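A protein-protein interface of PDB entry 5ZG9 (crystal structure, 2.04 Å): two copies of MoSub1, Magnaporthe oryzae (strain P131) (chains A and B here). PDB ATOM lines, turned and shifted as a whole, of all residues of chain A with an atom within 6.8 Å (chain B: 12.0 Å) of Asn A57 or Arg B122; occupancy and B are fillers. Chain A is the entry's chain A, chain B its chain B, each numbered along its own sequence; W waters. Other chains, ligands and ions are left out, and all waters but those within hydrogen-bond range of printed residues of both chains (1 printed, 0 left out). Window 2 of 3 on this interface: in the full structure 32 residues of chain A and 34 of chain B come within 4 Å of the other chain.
Of the 14 printed residues of chain B, 4 touch a printed residue of chain A.
Hydrophobic or aromatic side chains of chain B that line the printed part of chain A: His B124.
Of the 19 printed residues of chain A, 6 touch a printed residue of chain B.
No position is printed for both chains.
Of the 9 pairs that touch across the chains among the printed residues, none has its exchanged pair printed and touching as well.
The backbone NH (N) of Asn A57 lies within hydrogen-bond range of the side-chain carboxylate (OD1) of Asp A53, 3.0 Å away.
The backbone carbonyl oxygen (O) of Pro A58 is in hydrogen-bond range of the backbone NH (N) of Ile A70.
N of Phe A78 sits at hydrogen-bond distance from O of Ser A71.
The guanidinium group of Arg B122 is in salt-bridge range of the side-chain carboxylate of Glu B118 (3.2 Å).
O of Leu B119 lies within hydrogen-bond range of N of His B124, at 3.1 Å.
Water W1 lies within hydrogen-bond range of the side-chain carboxylate of Asp A77, the side-chain amide nitrogen of Gln A72 and the guanidinium group of Arg B122.
Among the printed residues, pairs that only touch across the chains: Asn A57 with Arg B122 (3.9 Å), Pro A58 with Arg B122 (3.8 Å), Ile A70 with Ile B115 (3.7 Å), Ile A70 with Glu B118 (3.5 Å), Ile A70 with Arg B122 (3.5 Å), Ser A71 with Arg B122 (3.9 Å) and Gln A72 with Arg B122 (3.8 Å).
Of chain B, only Arg B122 (3.9 Å) comes within 4 Å of Asn A57.
Arg B122 touches just these residues of chain A: Asn A57, Pro A58, Ile A70, Ser A71, Gln A72 and Asp A77.
No residue of chain B comes within 4 Å of Asp A53.
No residue of chain B comes within 4 Å of Ala A54.
No residue of chain B comes within 4 Å of Glu A55.
No residue of chain B comes within 4 Å of Gly A56.
No residue of chain B comes within 4 Å of Phe A59.
Ser A71 touches just one residue of chain B: Arg B122 (3.9 Å).
Of the printed residues of chain A, Glu B118 touches Ile A70.
Of the printed residues of chain A, Ile B115 touches Ile A70 (3.7 Å).
Printed residues of chain A within 4 Å of His B124: Asp A77.
The nearest residue of chain B that does not touch Asn A57 is Glu B118 (7.4 Å).
The side-chain carboxylate (OD1) of Asp A77 is in salt-bridge range of the guanidinium group (NH1) of Arg B122 (2.8 Å).
A ring nitrogen (NE2) of His B124 sits at hydrogen-bond distance from the side-chain carboxylate of Asp A77.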
ATOM      1  N   SER A  50     -26.644   8.711 -18.842  1.00  0.00           N
ATOM      2  CA  SER A  50     -25.443   8.302 -19.560  1.00  0.00           C
ATOM      3  C   SER A  50     -25.607   8.504 -21.061  1.00  0.00           C
ATOM      4  O   SER A  50     -26.641   8.972 -21.520  1.00  0.00           O
ATOM      5  CB  SER A  50     -25.140   6.825 -19.298  1.00  0.00           C
ATOM      6  OG  SER A  50     -25.915   5.996 -20.150  1.00  0.00           O
ATOM      7  N   GLN A  51     -24.574   8.154 -21.817  1.00  0.00           N
ATOM      8  CA  GLN A  51     -24.680   8.087 -23.262  1.00  0.00           C
ATOM      9  C   GLN A  51     -25.272   6.733 -23.621  1.00  0.00           C
ATOM     10  O   GLN A  51     -25.173   5.769 -22.849  1.00  0.00           O
ATOM     11  CB  GLN A  51     -23.303   8.221 -23.912  1.00  0.00           C
ATOM     12  CG  GLN A  51     -22.738   9.625 -23.905  1.00  0.00           C
ATOM     13  CD  GLN A  51     -22.408  10.098 -25.301  1.00  0.00           C
ATOM     14  OE1 GLN A  51     -21.271   9.965 -25.759  1.00  0.00           O
ATOM     15  NE2 GLN A  51     -23.409  10.635 -26.000  1.00  0.00           N
ATOM     16  N   VAL A  52     -25.890   6.669 -24.789  1.00  0.00           N
ATOM     17  CA  VAL A  52     -26.523   5.451 -25.267  1.00  0.00           C
ATOM     18  C   VAL A  52     -26.130   5.247 -26.715  1.00  0.00           C
ATOM     19  O   VAL A  52     -26.281   6.180 -27.521  1.00  0.00           O
ATOM     20  CB  VAL A  52     -28.049   5.591 -25.197  1.00  0.00           C
ATOM     21  CG1 VAL A  52     -28.707   4.399 -25.788  1.00  0.00           C
ATOM     22  CG2 VAL A  52     -28.488   5.771 -23.758  1.00  0.00           C
ATOM     23  N   ASP A  53     -25.648   4.049 -27.060  1.00  0.00           N
ATOM     24  CA  ASP A  53     -25.306   3.753 -28.462  1.00  0.00           C
ATOM     25  C   ASP A  53     -26.529   3.521 -29.358  1.00  0.00           C
ATOM     26  O   ASP A  53     -27.664   3.477 -28.874  1.00  0.00           O
ATOM     27  CB  ASP A  53     -24.316   2.581 -28.580  1.00  0.00           C
ATOM     28  CG  ASP A  53     -24.865   1.275 -28.015  1.00  0.00           C
ATOM     29  OD1 ASP A  53     -26.071   0.988 -28.192  1.00  0.00           O
ATOM     30  OD2 ASP A  53     -24.081   0.523 -27.390  1.00  0.00           O
ATOM     31  N   ALA A  54     -26.294   3.337 -30.655  1.00  0.00           N
ATOM     32  CA  ALA A  54     -27.393   3.198 -31.617  1.00  0.00           C
ATOM     33  C   ALA A  54     -28.251   1.953 -31.391  1.00  0.00           C
ATOM     34  O   ALA A  54     -29.330   1.832 -31.961  1.00  0.00           O
ATOM     35  CB  ALA A  54     -26.864   3.223 -33.048  1.00  0.00           C
ATOM     36  N   GLU A  55     -27.760   1.030 -30.572  1.00  0.00           N
ATOM     37  CA  GLU A  55     -28.523  -0.166 -30.243  1.00  0.00           C
ATOM     38  C   GLU A  55     -29.364   0.009 -28.973  1.00  0.00           C
ATOM     39  O   GLU A  55     -30.061  -0.916 -28.563  1.00  0.00           O
ATOM     40  CB  GLU A  55     -27.584  -1.366 -30.096  1.00  0.00           C
ATOM     41  CG  GLU A  55     -26.648  -1.571 -31.285  1.00  0.00           C
ATOM     42  CD  GLU A  55     -27.387  -1.638 -32.610  1.00  0.00           C
ATOM     43  OE1 GLU A  55     -28.063  -2.658 -32.868  1.00  0.00           O
ATOM     44  OE2 GLU A  55     -27.294  -0.667 -33.395  1.00  0.00           O
ATOM     45  N   GLY A  56     -29.297   1.189 -28.357  1.00  0.00           N
ATOM     46  CA  GLY A  56     -30.060   1.461 -27.152  1.00  0.00           C
ATOM     47  C   GLY A  56     -29.304   1.149 -25.868  1.00  0.00           C
ATOM     48  O   GLY A  56     -29.856   1.269 -24.773  1.00  0.00           O
ATOM     49  N   ASN A  57     -28.033   0.784 -25.985  1.00  0.00           N
ATOM     50  CA  ASN A  57     -27.276   0.345 -24.812  1.00  0.00           C
ATOM     51  C   ASN A  57     -26.344   1.390 -24.215  1.00  0.00           C
ATOM     52  O   ASN A  57     -25.621   2.077 -24.945  1.00  0.00           O
ATOM     53  CB  ASN A  57     -26.498  -0.922 -25.142  1.00  0.00           C
ATOM     54  CG  ASN A  57     -27.413  -2.067 -25.535  1.00  0.00           C
ATOM     55  OD1 ASN A  57     -27.242  -2.685 -26.585  1.00  0.00           O
ATOM     56  ND2 ASN A  57     -28.410  -2.340 -24.693  1.00  0.00           N
ATOM     57  N   PRO A  58     -26.343   1.497 -22.875  1.00  0.00           N
ATOM     58  CA  PRO A  58     -25.528   2.517 -22.208  1.00  0.00           C
ATOM     59  C   PRO A  58     -24.055   2.200 -22.348  1.00  0.00           C
ATOM     60  O   PRO A  58     -23.666   1.025 -22.426  1.00  0.00           O
ATOM     61  CB  PRO A  58     -25.965   2.430 -20.746  1.00  0.00           C
ATOM     62  CG  PRO A  58     -26.475   1.023 -20.583  1.00  0.00           C
ATOM     63  CD  PRO A  58     -27.075   0.643 -21.919  1.00  0.00           C
ATOM     64  N   PHE A  59     -23.242   3.248 -22.429  1.00  0.00           N
ATOM     65  CA  PHE A  59     -21.794   3.078 -22.505  1.00  0.00           C
ATOM     66  C   PHE A  59     -21.069   4.261 -21.874  1.00  0.00           C
ATOM     67  O   PHE A  59     -21.613   5.370 -21.776  1.00  0.00           O
ATOM     68  CB  PHE A  59     -21.331   2.835 -23.963  1.00  0.00           C
ATOM     69  CG  PHE A  59     -21.372   4.062 -24.837  1.00  0.00           C
ATOM     70  CD1 PHE A  59     -20.299   4.948 -24.869  1.00  0.00           C
ATOM     71  CD2 PHE A  59     -22.479   4.318 -25.645  1.00  0.00           C
ATOM     72  CE1 PHE A  59     -20.335   6.088 -25.670  1.00  0.00           C
ATOM     73  CE2 PHE A  59     -22.511   5.440 -26.460  1.00  0.00           C
ATOM     74  CZ  PHE A  59     -21.436   6.331 -26.467  1.00  0.00           C
ATOM     75  N   ARG A  67     -14.786   2.011 -25.505  1.00  0.00           N
ATOM     76  CA  ARG A  67     -15.962   2.125 -24.658  1.00  0.00           C
ATOM     77  C   ARG A  67     -16.035   0.944 -23.697  1.00  0.00           C
ATOM     78  O   ARG A  67     -15.543  -0.153 -24.002  1.00  0.00           O
ATOM     79  CB  ARG A  67     -17.213   2.091 -25.522  1.00  0.00           C
ATOM     80  CG  ARG A  67     -17.307   3.216 -26.543  1.00  0.00           C
ATOM     81  CD  ARG A  67     -18.616   3.124 -27.309  1.00  0.00           C
ATOM     82  NE  ARG A  67     -18.802   4.269 -28.193  1.00  0.00           N
ATOM     83  CZ  ARG A  67     -19.824   4.403 -29.029  1.00  0.00           C
ATOM     84  NH1 ARG A  67     -20.766   3.465 -29.086  1.00  0.00           N
ATOM     85  NH2 ARG A  67     -19.904   5.478 -29.797  1.00  0.00           N
ATOM     86  N   GLY A  69     -19.392  -0.809 -21.957  1.00  0.00           N
ATOM     87  CA  GLY A  69     -20.839  -0.689 -22.079  1.00  0.00           C
ATOM     88  C   GLY A  69     -21.522  -1.956 -21.622  1.00  0.00           C
ATOM     89  O   GLY A  69     -20.875  -3.002 -21.463  1.00  0.00           O
ATOM     90  N   ILE A  70     -22.824  -1.874 -21.392  1.00  0.00           N
ATOM     91  CA  ILE A  70     -23.564  -3.045 -20.965  1.00  0.00           C
ATOM     92  C   ILE A  70     -24.578  -3.414 -22.028  1.00  0.00           C
ATOM     93  O   ILE A  70     -25.376  -2.572 -22.465  1.00  0.00           O
ATOM     94  CB  ILE A  70     -24.297  -2.800 -19.652  1.00  0.00           C
ATOM     95  CG1 ILE A  70     -23.292  -2.523 -18.533  1.00  0.00           C
ATOM     96  CG2 ILE A  70     -25.178  -4.013 -19.299  1.00  0.00           C
ATOM     97  CD1 ILE A  70     -23.927  -1.906 -17.325  1.00  0.00           C
ATOM     98  N   SER A  71     -24.553  -4.679 -22.427  1.00  0.00           N
ATOM     99  CA  SER A  71     -25.436  -5.166 -23.469  1.00  0.00           C
ATOM    100  C   SER A  71     -26.119  -6.469 -23.035  1.00  0.00           C
ATOM    101  O   SER A  71     -25.525  -7.275 -22.310  1.00  0.00           O
ATOM    102  CB  SER A  71     -24.628  -5.381 -24.757  1.00  0.00           C
ATOM    103  OG  SER A  71     -25.410  -6.035 -25.737  1.00  0.00           O
ATOM    104  N   GLN A  72     -27.362  -6.672 -23.471  1.00  0.00           N
ATOM    105  CA  GLN A  72     -28.054  -7.934 -23.225  1.00  0.00           C
ATOM    106  C   GLN A  72     -28.071  -8.749 -24.514  1.00  0.00           C
ATOM    107  O   GLN A  72     -28.536  -8.266 -25.548  1.00  0.00           O
ATOM    108  CB  GLN A  72     -29.489  -7.714 -22.738  1.00  0.00           C
ATOM    109  CG  GLN A  72     -30.196  -9.027 -22.366  1.00  0.00           C
ATOM    110  CD  GLN A  72     -31.693  -8.875 -22.160  1.00  0.00           C
ATOM    111  OE1 GLN A  72     -32.459  -8.774 -23.121  1.00  0.00           O
ATOM    112  NE2 GLN A  72     -32.118  -8.869 -20.904  1.00  0.00           N
ATOM    113  N   PHE A  73     -27.568  -9.980 -24.451  1.00  0.00           N
ATOM    114  CA  PHE A  73     -27.453 -10.833 -25.636  1.00  0.00           C
ATOM    115  C   PHE A  73     -27.741 -12.291 -25.268  1.00  0.00           C
ATOM    116  O   PHE A  73     -27.092 -12.848 -24.383  1.00  0.00           O
ATOM    117  CB  PHE A  73     -26.045 -10.705 -26.217  1.00  0.00           C
ATOM    118  CG  PHE A  73     -25.821 -11.501 -27.478  1.00  0.00           C
ATOM    119  CD1 PHE A  73     -26.410 -11.113 -28.678  1.00  0.00           C
ATOM    120  CD2 PHE A  73     -24.976 -12.611 -27.473  1.00  0.00           C
ATOM    121  CE1 PHE A  73     -26.185 -11.837 -29.846  1.00  0.00           C
ATOM    122  CE2 PHE A  73     -24.745 -13.334 -28.635  1.00  0.00           C
ATOM    123  CZ  PHE A  73     -25.354 -12.946 -29.822  1.00  0.00           C
ATOM    124  N   MET A  76     -28.664 -12.785 -21.541  1.00  0.00           N
ATOM    125  CA  MET A  76     -27.738 -12.463 -20.467  1.00  0.00           C
ATOM    126  C   MET A  76     -27.036 -11.144 -20.713  1.00  0.00           C
ATOM    127  O   MET A  76     -26.866 -10.711 -21.869  1.00  0.00           O
ATOM    128  CB  MET A  76     -26.749 -13.594 -20.157  1.00  0.00           C
ATOM    129  CG  MET A  76     -26.137 -14.287 -21.338  1.00  0.00           C
ATOM    130  SD  MET A  76     -25.325 -15.813 -20.777  1.00  0.00           S
ATOM    131  CE  MET A  76     -23.969 -15.107 -19.828  1.00  0.00           C
ATOM    132  N   ASP A  77     -26.655 -10.503 -19.610  1.00  0.00           N
ATOM    133  CA  ASP A  77     -25.979  -9.217 -19.653  1.00  0.00           C
ATOM    134  C   ASP A  77     -24.486  -9.403 -19.773  1.00  0.00           C
ATOM    135  O   ASP A  77     -23.904 -10.285 -19.145  1.00  0.00           O
ATOM    136  CB  ASP A  77     -26.295  -8.426 -18.393  1.00  0.00           C
ATOM    137  CG  ASP A  77     -27.741  -8.020 -18.326  1.00  0.00           C
ATOM    138  OD1 ASP A  77     -28.190  -7.348 -19.277  1.00  0.00           O
ATOM    139  OD2 ASP A  77     -28.430  -8.393 -17.349  1.00  0.00           O
ATOM    140  N   PHE A  78     -23.869  -8.558 -20.585  1.00  0.00           N
ATOM    141  CA  PHE A  78     -22.437  -8.605 -20.776  1.00  0.00           C
ATOM    142  C   PHE A  78     -21.871  -7.221 -20.542  1.00  0.00           C
ATOM    143  O   PHE A  78     -22.487  -6.211 -20.940  1.00  0.00           O
ATOM    144  CB  PHE A  78     -22.120  -9.043 -22.208  1.00  0.00           C
ATOM    145  CG  PHE A  78     -22.402 -10.483 -22.453  1.00  0.00           C
ATOM    146  CD1 PHE A  78     -21.458 -11.445 -22.118  1.00  0.00           C
ATOM    147  CD2 PHE A  78     -23.628 -10.887 -22.961  1.00  0.00           C
ATOM    148  CE1 PHE A  78     -21.715 -12.806 -22.308  1.00  0.00           C
ATOM    149  CE2 PHE A  78     -23.904 -12.254 -23.161  1.00  0.00           C
ATOM    150  CZ  PHE A  78     -22.944 -13.215 -22.827  1.00  0.00           C
ATOM    151  N   PRO B 113     -19.072   2.881 -10.708  1.00  0.00           N
ATOM    152  CA  PRO B 113     -20.323   3.014  -9.952  1.00  0.00           C
ATOM    153  C   PRO B 113     -21.526   3.034 -10.887  1.00  0.00           C
ATOM    154  O   PRO B 113     -22.524   2.368 -10.594  1.00  0.00           O
ATOM    155  CB  PRO B 113     -20.166   4.360  -9.240  1.00  0.00           C
ATOM    156  CG  PRO B 113     -18.686   4.565  -9.140  1.00  0.00           C
ATOM    157  CD  PRO B 113     -18.142   3.988 -10.425  1.00  0.00           C
ATOM    158  N   ALA B 114     -21.429   3.759 -12.000  1.00  0.00           N
ATOM    159  CA  ALA B 114     -22.517   3.794 -12.978  1.00  0.00           C
ATOM    160  C   ALA B 114     -22.775   2.427 -13.642  1.00  0.00           C
ATOM    161  O   ALA B 114     -23.930   2.060 -13.873  1.00  0.00           O
ATOM    162  CB  ALA B 114     -22.272   4.869 -14.019  1.00  0.00           C
ATOM    163  N   ILE B 115     -21.714   1.676 -13.943  1.00  0.00           N
ATOM    164  CA  ILE B 115     -21.867   0.306 -14.433  1.00  0.00           C
ATOM    165  C   ILE B 115     -22.571  -0.544 -13.381  1.00  0.00           C
ATOM    166  O   ILE B 115     -23.499  -1.306 -13.690  1.00  0.00           O
ATOM    167  CB  ILE B 115     -20.494  -0.344 -14.751  1.00  0.00           C
ATOM    168  CG1 ILE B 115     -19.867   0.324 -15.976  1.00  0.00           C
ATOM    169  CG2 ILE B 115     -20.643  -1.839 -15.017  1.00  0.00           C
ATOM    170  CD1 ILE B 115     -18.366   0.148 -16.047  1.00  0.00           C
ATOM    171  N   ASN B 116     -22.134  -0.420 -12.130  1.00  0.00           N
ATOM    172  CA  ASN B 116     -22.717  -1.232 -11.076  1.00  0.00           C
ATOM    173  C   ASN B 116     -24.186  -0.915 -10.927  1.00  0.00           C
ATOM    174  O   ASN B 116     -25.024  -1.819 -10.842  1.00  0.00           O
ATOM    175  CB  ASN B 116     -21.959  -1.044  -9.760  1.00  0.00           C
ATOM    176  CG  ASN B 116     -20.572  -1.686  -9.799  1.00  0.00           C
ATOM    177  OD1 ASN B 116     -20.155  -2.234 -10.828  1.00  0.00           O
ATOM    178  ND2 ASN B 116     -19.851  -1.611  -8.685  1.00  0.00           N
ATOM    179  N   ALA B 117     -24.498   0.374 -10.933  1.00  0.00           N
ATOM    180  CA  ALA B 117     -25.881   0.837 -10.786  1.00  0.00           C
ATOM    181  C   ALA B 117     -26.790   0.311 -11.911  1.00  0.00           C
ATOM    182  O   ALA B 117     -27.931  -0.108 -11.663  1.00  0.00           O
ATOM    183  CB  ALA B 117     -25.925   2.349 -10.710  1.00  0.00           C
ATOM    184  N   GLU B 118     -26.277   0.314 -13.139  1.00  0.00           N
ATOM    185  CA  GLU B 118     -27.031  -0.229 -14.267  1.00  0.00           C
ATOM    186  C   GLU B 118     -27.282  -1.730 -14.095  1.00  0.00           C
ATOM    187  O   GLU B 118     -28.416  -2.202 -14.266  1.00  0.00           O
ATOM    188  CB  GLU B 118     -26.300   0.027 -15.584  1.00  0.00           C
ATOM    189  CG  GLU B 118     -27.071  -0.456 -16.815  1.00  0.00           C
ATOM    190  CD  GLU B 118     -28.365   0.309 -17.023  1.00  0.00           C
ATOM    191  OE1 GLU B 118     -28.429   1.487 -16.611  1.00  0.00           O
ATOM    192  OE2 GLU B 118     -29.316  -0.269 -17.594  1.00  0.00           O
ATOM    193  N   LEU B 119     -26.231  -2.475 -13.758  1.00  0.00           N
ATOM    194  CA  LEU B 119     -26.382  -3.909 -13.517  1.00  0.00           C
ATOM    195  C   LEU B 119     -27.408  -4.192 -12.417  1.00  0.00           C
ATOM    196  O   LEU B 119     -28.279  -5.047 -12.602  1.00  0.00           O
ATOM    197  CB  LEU B 119     -25.038  -4.570 -13.210  1.00  0.00           C
ATOM    198  CG  LEU B 119     -24.039  -4.640 -14.371  1.00  0.00           C
ATOM    199  CD1 LEU B 119     -22.676  -5.162 -13.922  1.00  0.00           C
ATOM    200  CD2 LEU B 119     -24.582  -5.519 -15.471  1.00  0.00           C
ATOM    201  N   ARG B 120     -27.328  -3.472 -11.292  1.00  0.00           N
ATOM    202  CA  ARG B 120     -28.331  -3.622 -10.243  1.00  0.00           C
ATOM    203  C   ARG B 120     -29.729  -3.335 -10.782  1.00  0.00           C
ATOM    204  O   ARG B 120     -30.693  -4.001 -10.395  1.00  0.00           O
ATOM    205  CB  ARG B 120     -28.043  -2.716  -9.040  1.00  0.00           C
ATOM    206  CG  ARG B 120     -26.791  -3.085  -8.283  1.00  0.00           C
ATOM    207  CD  ARG B 120     -26.658  -2.311  -6.980  1.00  0.00           C
ATOM    208  NE  ARG B 120     -25.267  -2.311  -6.537  1.00  0.00           N
ATOM    209  CZ  ARG B 120     -24.423  -1.309  -6.761  1.00  0.00           C
ATOM    210  NH1 ARG B 120     -24.838  -0.220  -7.397  1.00  0.00           N
ATOM    211  NH2 ARG B 120     -23.167  -1.390  -6.340  1.00  0.00           N
ATOM    212  N   SER B 121     -29.842  -2.361 -11.682  1.00  0.00           N
ATOM    213  CA  SER B 121     -31.149  -2.042 -12.264  1.00  0.00           C
ATOM    214  C   SER B 121     -31.649  -3.200 -13.130  1.00  0.00           C
ATOM    215  O   SER B 121     -32.853  -3.441 -13.235  1.00  0.00           O
ATOM    216  CB  SER B 121     -31.086  -0.747 -13.075  1.00  0.00           C
ATOM    217  OG  SER B 121     -32.385  -0.326 -13.454  1.00  0.00           O
ATOM    218  N   ARG B 122     -30.716  -3.929 -13.733  1.00  0.00           N
ATOM    219  CA  ARG B 122     -31.073  -5.120 -14.490  1.00  0.00           C
ATOM    220  C   ARG B 122     -31.177  -6.374 -13.607  1.00  0.00           C
ATOM    221  O   ARG B 122     -31.218  -7.493 -14.118  1.00  0.00           O
ATOM    222  CB  ARG B 122     -30.073  -5.339 -15.625  1.00  0.00           C
ATOM    223  CG  ARG B 122     -30.120  -4.241 -16.674  1.00  0.00           C
ATOM    224  CD  ARG B 122     -28.965  -4.357 -17.653  1.00  0.00           C
ATOM    225  NE  ARG B 122     -29.040  -3.317 -18.676  1.00  0.00           N
ATOM    226  CZ  ARG B 122     -28.801  -3.524 -19.964  1.00  0.00           C
ATOM    227  NH1 ARG B 122     -28.465  -4.737 -20.384  1.00  0.00           N
ATOM    228  NH2 ARG B 122     -28.893  -2.524 -20.832  1.00  0.00           N
ATOM    229  N   GLY B 123     -31.212  -6.184 -12.289  1.00  0.00           N
ATOM    230  CA  GLY B 123     -31.441  -7.287 -11.370  1.00  0.00           C
ATOM    231  C   GLY B 123     -30.251  -8.123 -10.911  1.00  0.00           C
ATOM    232  O   GLY B 123     -30.441  -9.246 -10.430  1.00  0.00           O
ATOM    233  N   HIS B 124     -29.032  -7.604 -11.037  1.00  0.00           N
ATOM    234  CA  HIS B 124     -27.869  -8.322 -10.504  1.00  0.00           C
ATOM    235  C   HIS B 124     -27.410  -7.750  -9.164  1.00  0.00           C
ATOM    236  O   HIS B 124     -27.680  -6.592  -8.863  1.00  0.00           O
ATOM    237  CB  HIS B 124     -26.719  -8.296 -11.504  1.00  0.00           C
ATOM    238  CG  HIS B 124     -27.064  -8.897 -12.831  1.00  0.00           C
ATOM    239  ND1 HIS B 124     -26.952 -10.247 -13.087  1.00  0.00           N
ATOM    240  CD2 HIS B 124     -27.512  -8.328 -13.976  1.00  0.00           C
ATOM    241  CE1 HIS B 124     -27.317 -10.484 -14.335  1.00  0.00           C
ATOM    242  NE2 HIS B 124     -27.661  -9.337 -14.896  1.00  0.00           N
ATOM    243  N   ASP B 125     -26.714  -8.560  -8.366  1.00  0.00           N
ATOM    244  CA  ASP B 125     -26.238  -8.122  -7.051  1.00  0.00           C
ATOM    245  C   ASP B 125     -24.734  -7.839  -7.022  1.00  0.00           C
ATOM    246  O   ASP B 125     -23.918  -8.762  -7.101  1.00  0.00           O
ATOM    247  CB  ASP B 125     -26.585  -9.160  -5.984  1.00  0.00           C
ATOM    248  CG  ASP B 125     -26.242  -8.686  -4.584  1.00  0.00           C
ATOM    249  OD1 ASP B 125     -26.063  -7.459  -4.397  1.00  0.00           O
ATOM    250  OD2 ASP B 125     -26.160  -9.537  -3.666  1.00  0.00           O
ATOM    251  N   ILE B 126     -24.372  -6.567  -6.888  1.00  0.00           N
ATOM    252  CA  ILE B 126     -22.967  -6.169  -6.898  1.00  0.00           C
ATOM    253  C   ILE B 126     -22.492  -5.731  -5.509  1.00  0.00           C
ATOM    254  O   ILE B 126     -23.063  -4.824  -4.904  1.00  0.00           O
ATOM    255  CB  ILE B 126     -22.714  -5.039  -7.913  1.00  0.00           C
ATOM    256  CG1 ILE B 126     -23.434  -5.332  -9.233  1.00  0.00           C
ATOM    257  CG2 ILE B 126     -21.213  -4.842  -8.139  1.00  0.00           C
ATOM    258  CD1 ILE B 126     -22.815  -6.456 -10.065  1.00  0.00           C
HETATM  259  O   HOH W   1     -30.831  -6.701 -19.058  1.00  0.00           O
